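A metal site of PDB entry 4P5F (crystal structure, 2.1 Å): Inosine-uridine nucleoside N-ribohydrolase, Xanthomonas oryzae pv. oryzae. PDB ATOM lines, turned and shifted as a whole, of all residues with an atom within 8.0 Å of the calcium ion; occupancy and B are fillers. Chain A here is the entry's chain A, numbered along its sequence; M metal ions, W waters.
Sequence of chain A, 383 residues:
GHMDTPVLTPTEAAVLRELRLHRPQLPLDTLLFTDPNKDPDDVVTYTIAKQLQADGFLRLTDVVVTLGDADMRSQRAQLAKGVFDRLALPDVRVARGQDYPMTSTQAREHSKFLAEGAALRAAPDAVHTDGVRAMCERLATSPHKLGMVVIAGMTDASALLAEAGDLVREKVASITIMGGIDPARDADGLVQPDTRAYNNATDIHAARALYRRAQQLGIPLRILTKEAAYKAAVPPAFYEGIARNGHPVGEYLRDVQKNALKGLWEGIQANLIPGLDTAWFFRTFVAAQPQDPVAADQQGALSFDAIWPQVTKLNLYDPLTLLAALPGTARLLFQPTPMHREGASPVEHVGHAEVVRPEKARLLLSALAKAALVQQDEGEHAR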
ATOM      1  N   PHE A  33      16.037  -0.161  12.905  1.00  0.00           N
ATOM      2  CA  PHE A  33      16.771   0.748  13.776  1.00  0.00           C
ATOM      3  C   PHE A  33      15.779   1.379  14.725  1.00  0.00           C
ATOM      4  O   PHE A  33      14.858   2.078  14.299  1.00  0.00           O
ATOM      5  CB  PHE A  33      17.495   1.808  12.938  1.00  0.00           C
ATOM      6  CG  PHE A  33      18.448   1.230  11.942  1.00  0.00           C
ATOM      7  CD1 PHE A  33      17.986   0.767  10.718  1.00  0.00           C
ATOM      8  CD2 PHE A  33      19.802   1.114  12.230  1.00  0.00           C
ATOM      9  CE1 PHE A  33      18.882   0.219   9.791  1.00  0.00           C
ATOM     10  CE2 PHE A  33      20.685   0.549  11.296  1.00  0.00           C
ATOM     11  CZ  PHE A  33      20.212   0.109  10.097  1.00  0.00           C
ATOM     12  N   THR A  34      15.981   1.161  16.039  1.00  0.00           N
ATOM     13  CA  THR A  34      14.893   1.325  16.990  1.00  0.00           C
ATOM     14  C   THR A  34      15.374   1.756  18.386  1.00  0.00           C
ATOM     15  O   THR A  34      16.531   1.540  18.732  1.00  0.00           O
ATOM     16  CB  THR A  34      14.042   0.010  17.001  1.00  0.00           C
ATOM     17  OG1 THR A  34      12.980   0.098  17.947  1.00  0.00           O
ATOM     18  CG2 THR A  34      14.909  -1.185  17.328  1.00  0.00           C
ATOM     19  N   ASP A  35      14.494   2.393  19.153  1.00  0.00           N
ATOM     20  CA  ASP A  35      14.828   2.888  20.487  1.00  0.00           C
ATOM     21  C   ASP A  35      13.703   2.586  21.492  1.00  0.00           C
ATOM     22  O   ASP A  35      12.998   3.481  21.951  1.00  0.00           O
ATOM     23  CB  ASP A  35      15.115   4.397  20.426  1.00  0.00           C
ATOM     24  CG  ASP A  35      13.936   5.207  19.855  1.00  0.00           C
ATOM     25  OD1 ASP A  35      13.037   4.592  19.265  1.00  0.00           O
ATOM     26  OD2 ASP A  35      13.910   6.451  19.979  1.00  0.00           O
ATOM     27  N   PRO A  36      13.509   1.291  21.824  1.00  0.00           N
ATOM     28  CA  PRO A  36      12.306   0.888  22.584  1.00  0.00           C
ATOM     29  C   PRO A  36      12.315   1.283  24.059  1.00  0.00           C
ATOM     30  O   PRO A  36      13.368   1.573  24.640  1.00  0.00           O
ATOM     31  CB  PRO A  36      12.314  -0.627  22.451  1.00  0.00           C
ATOM     32  CG  PRO A  36      13.753  -0.963  22.281  1.00  0.00           C
ATOM     33  CD  PRO A  36      14.291   0.116  21.408  1.00  0.00           C
ATOM     34  N   ASN A  37      11.115   1.289  24.642  1.00  0.00           N
ATOM     35  CA  ASN A  37      10.914   1.441  26.082  1.00  0.00           C
ATOM     36  C   ASN A  37      11.108   2.863  26.615  1.00  0.00           C
ATOM     37  O   ASN A  37      11.502   3.056  27.773  1.00  0.00           O
ATOM     38  CB  ASN A  37      11.753   0.419  26.880  1.00  0.00           C
ATOM     39  CG  ASN A  37      11.162   0.124  28.251  1.00  0.00           C
ATOM     40  OD1 ASN A  37       9.959  -0.095  28.379  1.00  0.00           O
ATOM     41  ND2 ASN A  37      12.011   0.098  29.277  1.00  0.00           N
ATOM     42  N   LYS A  38      10.836   3.854  25.785  1.00  0.00           N
ATOM     43  CA  LYS A  38      10.542   5.186  26.264  1.00  0.00           C
ATOM     44  C   LYS A  38       9.116   5.602  25.879  1.00  0.00           C
ATOM     45  O   LYS A  38       8.625   6.641  26.320  1.00  0.00           O
ATOM     46  CB  LYS A  38      11.606   6.218  25.843  1.00  0.00           C
ATOM     47  CG  LYS A  38      11.969   6.229  24.374  1.00  0.00           C
ATOM     48  CD  LYS A  38      11.044   7.111  23.581  1.00  0.00           C
ATOM     49  CE  LYS A  38      11.416   7.100  22.103  1.00  0.00           C
ATOM     50  NZ  LYS A  38      10.424   7.850  21.312  1.00  0.00           N
ATOM     51  N   ASP A  39       8.468   4.784  25.061  1.00  0.00           N
ATOM     52  CA  ASP A  39       7.043   4.922  24.746  1.00  0.00           C
ATOM     53  C   ASP A  39       6.567   3.570  24.173  1.00  0.00           C
ATOM     54  O   ASP A  39       7.388   2.660  24.084  1.00  0.00           O
ATOM     55  CB  ASP A  39       6.779   6.108  23.802  1.00  0.00           C
ATOM     56  CG  ASP A  39       7.531   6.016  22.495  1.00  0.00           C
ATOM     57  OD1 ASP A  39       7.741   4.905  21.972  1.00  0.00           O
ATOM     58  OD2 ASP A  39       7.912   7.081  21.961  1.00  0.00           O
ATOM     59  N   PRO A  40       5.277   3.412  23.814  1.00  0.00           N
ATOM     60  CA  PRO A  40       4.863   2.091  23.302  1.00  0.00           C
ATOM     61  C   PRO A  40       5.280   1.809  21.849  1.00  0.00           C
ATOM     62  O   PRO A  40       5.324   0.641  21.455  1.00  0.00           O
ATOM     63  CB  PRO A  40       3.329   2.153  23.347  1.00  0.00           C
ATOM     64  CG  PRO A  40       2.997   3.291  24.265  1.00  0.00           C
ATOM     65  CD  PRO A  40       4.109   4.269  24.094  1.00  0.00           C
ATOM     66  N   ASP A  41       5.575   2.847  21.091  1.00  0.00           N
ATOM     67  CA  ASP A  41       5.645   2.781  19.624  1.00  0.00           C
ATOM     68  C   ASP A  41       6.475   1.634  19.037  1.00  0.00           C
ATOM     69  O   ASP A  41       5.968   0.865  18.221  1.00  0.00           O
ATOM     70  CB  ASP A  41       6.126   4.131  19.067  1.00  0.00           C
ATOM     71  CG  ASP A  41       5.198   4.664  17.985  1.00  0.00           C
ATOM     72  OD1 ASP A  41       4.051   4.175  17.910  1.00  0.00           O
ATOM     73  OD2 ASP A  41       5.609   5.551  17.210  1.00  0.00           O
ATOM     74  N   ASP A  42       7.729   1.537  19.464  1.00  0.00           N
ATOM     75  CA  ASP A  42       8.649   0.532  18.926  1.00  0.00           C
ATOM     76  C   ASP A  42       8.196  -0.900  19.208  1.00  0.00           C
ATOM     77  O   ASP A  42       8.361  -1.785  18.376  1.00  0.00           O
ATOM     78  CB  ASP A  42      10.079   0.733  19.465  1.00  0.00           C
ATOM     79  CG  ASP A  42      10.668   2.067  19.057  1.00  0.00           C
ATOM     80  OD1 ASP A  42      10.229   3.095  19.626  1.00  0.00           O
ATOM     81  OD2 ASP A  42      11.558   2.107  18.168  1.00  0.00           O
ATOM     82  N   VAL A  43       7.657  -1.146  20.394  1.00  0.00           N
ATOM     83  CA  VAL A  43       7.257  -2.514  20.727  1.00  0.00           C
ATOM     84  C   VAL A  43       5.973  -2.872  19.983  1.00  0.00           C
ATOM     85  O   VAL A  43       5.774  -4.036  19.616  1.00  0.00           O
ATOM     86  CB  VAL A  43       7.187  -2.744  22.236  1.00  0.00           C
ATOM     87  CG1 VAL A  43       6.592  -4.109  22.580  1.00  0.00           C
ATOM     88  CG2 VAL A  43       8.575  -2.630  22.812  1.00  0.00           C
ATOM     89  N   THR A  45       5.443  -1.970  16.988  1.00  0.00           N
ATOM     90  CA  THR A  45       6.035  -2.306  15.701  1.00  0.00           C
ATOM     91  C   THR A  45       6.600  -3.719  15.673  1.00  0.00           C
ATOM     92  O   THR A  45       6.378  -4.448  14.691  1.00  0.00           O
ATOM     93  CB  THR A  45       7.153  -1.311  15.317  1.00  0.00           C
ATOM     94  OG1 THR A  45       6.672   0.036  15.509  1.00  0.00           O
ATOM     95  CG2 THR A  45       7.564  -1.484  13.870  1.00  0.00           C
ATOM     96  N   TYR A  46       7.314  -4.122  16.726  1.00  0.00           N
ATOM     97  CA  TYR A  46       7.806  -5.493  16.828  1.00  0.00           C
ATOM     98  C   TYR A  46       6.623  -6.463  16.809  1.00  0.00           C
ATOM     99  O   TYR A  46       6.714  -7.534  16.230  1.00  0.00           O
ATOM    100  CB  TYR A  46       8.587  -5.759  18.132  1.00  0.00           C
ATOM    101  CG  TYR A  46       9.693  -4.787  18.474  1.00  0.00           C
ATOM    102  CD1 TYR A  46      10.261  -3.961  17.509  1.00  0.00           C
ATOM    103  CD2 TYR A  46      10.194  -4.728  19.759  1.00  0.00           C
ATOM    104  CE1 TYR A  46      11.282  -3.073  17.844  1.00  0.00           C
ATOM    105  CE2 TYR A  46      11.189  -3.857  20.109  1.00  0.00           C
ATOM    106  CZ  TYR A  46      11.737  -3.040  19.148  1.00  0.00           C
ATOM    107  OH  TYR A  46      12.734  -2.173  19.522  1.00  0.00           O
ATOM    108  N   THR A  66      19.353   2.143  19.558  1.00  0.00           N
ATOM    109  CA  THR A  66      19.956   3.406  19.921  1.00  0.00           C
ATOM    110  C   THR A  66      19.211   4.105  21.065  1.00  0.00           C
ATOM    111  O   THR A  66      18.272   3.530  21.655  1.00  0.00           O
ATOM    112  CB  THR A  66      20.051   4.362  18.694  1.00  0.00           C
ATOM    113  OG1 THR A  66      20.837   5.491  19.044  1.00  0.00           O
ATOM    114  CG2 THR A  66      18.640   4.814  18.231  1.00  0.00           C
ATOM    115  N   LEU A  67      19.633   5.340  21.352  1.00  0.00           N
ATOM    116  CA  LEU A  67      19.052   6.246  22.362  1.00  0.00           C
ATOM    117  C   LEU A  67      19.587   5.989  23.781  1.00  0.00           C
ATOM    118  O   LEU A  67      19.140   5.088  24.480  1.00  0.00           O
ATOM    119  CB  LEU A  67      17.512   6.255  22.342  1.00  0.00           C
ATOM    120  CG  LEU A  67      16.852   7.370  23.157  1.00  0.00           C
ATOM    121  CD1 LEU A  67      17.123   8.751  22.517  1.00  0.00           C
ATOM    122  CD2 LEU A  67      15.344   7.118  23.317  1.00  0.00           C
ATOM    123  N   VAL A 150      13.789   2.768   9.710  1.00  0.00           N
ATOM    124  CA  VAL A 150      14.347   3.604  10.759  1.00  0.00           C
ATOM    125  C   VAL A 150      13.227   4.202  11.600  1.00  0.00           C
ATOM    126  O   VAL A 150      12.461   5.032  11.123  1.00  0.00           O
ATOM    127  CB  VAL A 150      15.221   4.709  10.167  1.00  0.00           C
ATOM    128  CG1 VAL A 150      15.748   5.625  11.254  1.00  0.00           C
ATOM    129  CG2 VAL A 150      16.389   4.096   9.330  1.00  0.00           C
ATOM    130  N   ILE A 151      13.114   3.751  12.847  1.00  0.00           N
ATOM    131  CA  ILE A 151      12.103   4.274  13.763  1.00  0.00           C
ATOM    132  C   ILE A 151      12.737   4.877  15.044  1.00  0.00           C
ATOM    133  O   ILE A 151      12.155   4.820  16.125  1.00  0.00           O
ATOM    134  CB  ILE A 151      11.010   3.201  14.071  1.00  0.00           C
ATOM    135  CG1 ILE A 151      11.635   1.883  14.544  1.00  0.00           C
ATOM    136  CG2 ILE A 151      10.175   2.897  12.817  1.00  0.00           C
ATOM    137  CD1 ILE A 151      10.600   0.907  15.147  1.00  0.00           C
ATOM    138  N   ALA A 152      13.914   5.457  14.897  1.00  0.00           N
ATOM    139  CA  ALA A 152      14.667   6.021  16.026  1.00  0.00           C
ATOM    140  C   ALA A 152      15.734   6.951  15.481  1.00  0.00           C
ATOM    141  O   ALA A 152      15.804   7.126  14.260  1.00  0.00           O
ATOM    142  CB  ALA A 152      15.330   4.888  16.834  1.00  0.00           C
ATOM    143  N   GLY A 153      16.560   7.509  16.370  1.00  0.00           N
ATOM    144  CA  GLY A 153      17.706   8.303  15.965  1.00  0.00           C
ATOM    145  C   GLY A 153      18.529   7.577  14.908  1.00  0.00           C
ATOM    146  O   GLY A 153      18.471   6.354  14.820  1.00  0.00           O
ATOM    147  N   MET A 178      10.741   7.100  10.082  1.00  0.00           N
ATOM    148  CA  MET A 178       9.782   7.904  10.829  1.00  0.00           C
ATOM    149  C   MET A 178      10.532   9.163  11.219  1.00  0.00           C
ATOM    150  O   MET A 178      11.327   9.147  12.157  1.00  0.00           O
ATOM    151  CB  MET A 178       9.284   7.152  12.064  1.00  0.00           C
ATOM    152  CG  MET A 178       7.988   7.670  12.646  1.00  0.00           C
ATOM    153  SD  MET A 178       8.220   9.250  13.464  1.00  0.00           S
ATOM    154  CE  MET A 178       7.197  10.342  12.461  1.00  0.00           C
ATOM    155  N   TYR A 198      11.405  14.287  16.476  1.00  0.00           N
ATOM    156  CA  TYR A 198      12.116  13.529  17.513  1.00  0.00           C
ATOM    157  C   TYR A 198      13.258  12.644  16.989  1.00  0.00           C
ATOM    158  O   TYR A 198      14.357  12.703  17.514  1.00  0.00           O
ATOM    159  CB  TYR A 198      11.148  12.671  18.340  1.00  0.00           C
ATOM    160  CG  TYR A 198      11.800  12.013  19.544  1.00  0.00           C
ATOM    161  CD1 TYR A 198      12.475  10.803  19.408  1.00  0.00           C
ATOM    162  CD2 TYR A 198      11.763  12.604  20.796  1.00  0.00           C
ATOM    163  CE1 TYR A 198      13.088  10.208  20.475  1.00  0.00           C
ATOM    164  CE2 TYR A 198      12.376  12.005  21.887  1.00  0.00           C
ATOM    165  CZ  TYR A 198      13.032  10.801  21.712  1.00  0.00           C
ATOM    166  OH  TYR A 198      13.652  10.176  22.766  1.00  0.00           O
ATOM    167  N   ASN A 199      12.996  11.808  15.999  1.00  0.00           N
ATOM    168  CA  ASN A 199      14.038  10.914  15.523  1.00  0.00           C
ATOM    169  C   ASN A 199      15.209  11.628  14.860  1.00  0.00           C
ATOM    170  O   ASN A 199      16.360  11.187  14.975  1.00  0.00           O
ATOM    171  CB  ASN A 199      13.455   9.818  14.657  1.00  0.00           C
ATOM    172  CG  ASN A 199      12.627   8.847  15.455  1.00  0.00           C
ATOM    173  OD1 ASN A 199      12.839   8.674  16.661  1.00  0.00           O
ATOM    174  ND2 ASN A 199      11.666   8.215  14.803  1.00  0.00           N
ATOM    175  N   TYR A 317       3.088   6.050  15.396  1.00  0.00           N
ATOM    176  CA  TYR A 317       3.999   6.510  14.342  1.00  0.00           C
ATOM    177  C   TYR A 317       4.872   5.399  13.759  1.00  0.00           C
ATOM    178  O   TYR A 317       4.987   5.259  12.556  1.00  0.00           O
ATOM    179  CB  TYR A 317       4.920   7.601  14.851  1.00  0.00           C
ATOM    180  CG  TYR A 317       4.223   8.660  15.671  1.00  0.00           C
ATOM    181  CD1 TYR A 317       4.112   8.550  17.048  1.00  0.00           C
ATOM    182  CD2 TYR A 317       3.688   9.771  15.052  1.00  0.00           C
ATOM    183  CE1 TYR A 317       3.472   9.536  17.792  1.00  0.00           C
ATOM    184  CE2 TYR A 317       3.045  10.752  15.767  1.00  0.00           C
ATOM    185  CZ  TYR A 317       2.938  10.640  17.127  1.00  0.00           C
ATOM    186  OH  TYR A 317       2.284  11.651  17.801  1.00  0.00           O
ATOM    187  N   ASP A 318       5.491   4.628  14.628  1.00  0.00           N
ATOM    188  CA  ASP A 318       6.441   3.619  14.195  1.00  0.00           C
ATOM    189  C   ASP A 318       5.765   2.442  13.468  1.00  0.00           C
ATOM    190  O   ASP A 318       6.282   1.974  12.465  1.00  0.00           O
ATOM    191  CB  ASP A 318       7.309   3.125  15.368  1.00  0.00           C
ATOM    192  CG  ASP A 318       8.236   4.206  15.908  1.00  0.00           C
ATOM    193  OD1 ASP A 318       8.359   5.294  15.285  1.00  0.00           O
ATOM    194  OD2 ASP A 318       8.861   3.935  16.961  1.00  0.00           O
ATOM    195  N   PRO A 319       4.614   1.956  13.981  1.00  0.00           N
ATOM    196  CA  PRO A 319       3.936   0.885  13.243  1.00  0.00           C
ATOM    197  C   PRO A 319       3.511   1.288  11.822  1.00  0.00           C
ATOM    198  O   PRO A 319       3.658   0.494  10.877  1.00  0.00           O
ATOM    199  CB  PRO A 319       2.698   0.614  14.113  1.00  0.00           C
ATOM    200  CG  PRO A 319       3.132   0.938  15.464  1.00  0.00           C
ATOM    201  CD  PRO A 319       4.015   2.139  15.318  1.00  0.00           C
HETATM  202 CA    CA M   1      10.793   4.875  18.142  1.00  0.00          CA
HETATM  203  O   HOH W   1      11.785   7.149  18.756  1.00  0.00           O
HETATM  204  O   HOH W   2       8.926   5.931  19.492  1.00  0.00           O
HETATM  205  O   HOH W   3       9.787   7.109  16.602  1.00  0.00           O
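The side-chain hydroxyl of Thr 34 sits close to the side-chain carboxylate of Asp 42, at 2.5 Å.
The backbone NH (N) of Ile 151 lies within hydrogen-bond range of the backbone carbonyl oxygen (O) of Phe 33.
N of Asp 318 sits at hydrogen-bond distance from OD2 of Asp 41, 2.7 Å away.
The side-chain amino group (NZ) of Lys 38 is in salt-bridge range of the side-chain carboxylate (OD2) of Asp 35, 3.99 Å away.
Of the 25 residues printed, 4 come within 4 Å of the calcium ion.
The calcium ion is bound by the side-chain carboxylate (OD1) of Asp 42 (2.4 Å), the backbone carbonyl oxygen (O) of Ile 151 (2.4 Å), the side-chain carboxylate (OD2) of Asp 318 (2.5 Å), the side-chain carboxylate (OD1) of Asp 35 (2.5 Å), water W2 (2.5 Å), water W1 (2.6 Å), the side-chain carboxylate (OD2) of Asp 42 (2.9 Å) and water W3 (2.9 Å).
The calcium ion has eight donor atoms within binding distance.
Water W3 lies within hydrogen-bond range of OD1 of Asp 318 and ND2 of Asn 199.
Water W2 bridges the side-chain carboxylate of Asp 39 (2.9 Å) and the side-chain amino group of Lys 38 (3.0 Å).
Water W1 lies within hydrogen-bond range of the side-chain carboxylate of Asp 35 (2.5 Å), the side-chain amide oxygen of Asn 199 (2.8 Å) and the side-chain amino group of Lys 38 (3.0 Å).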
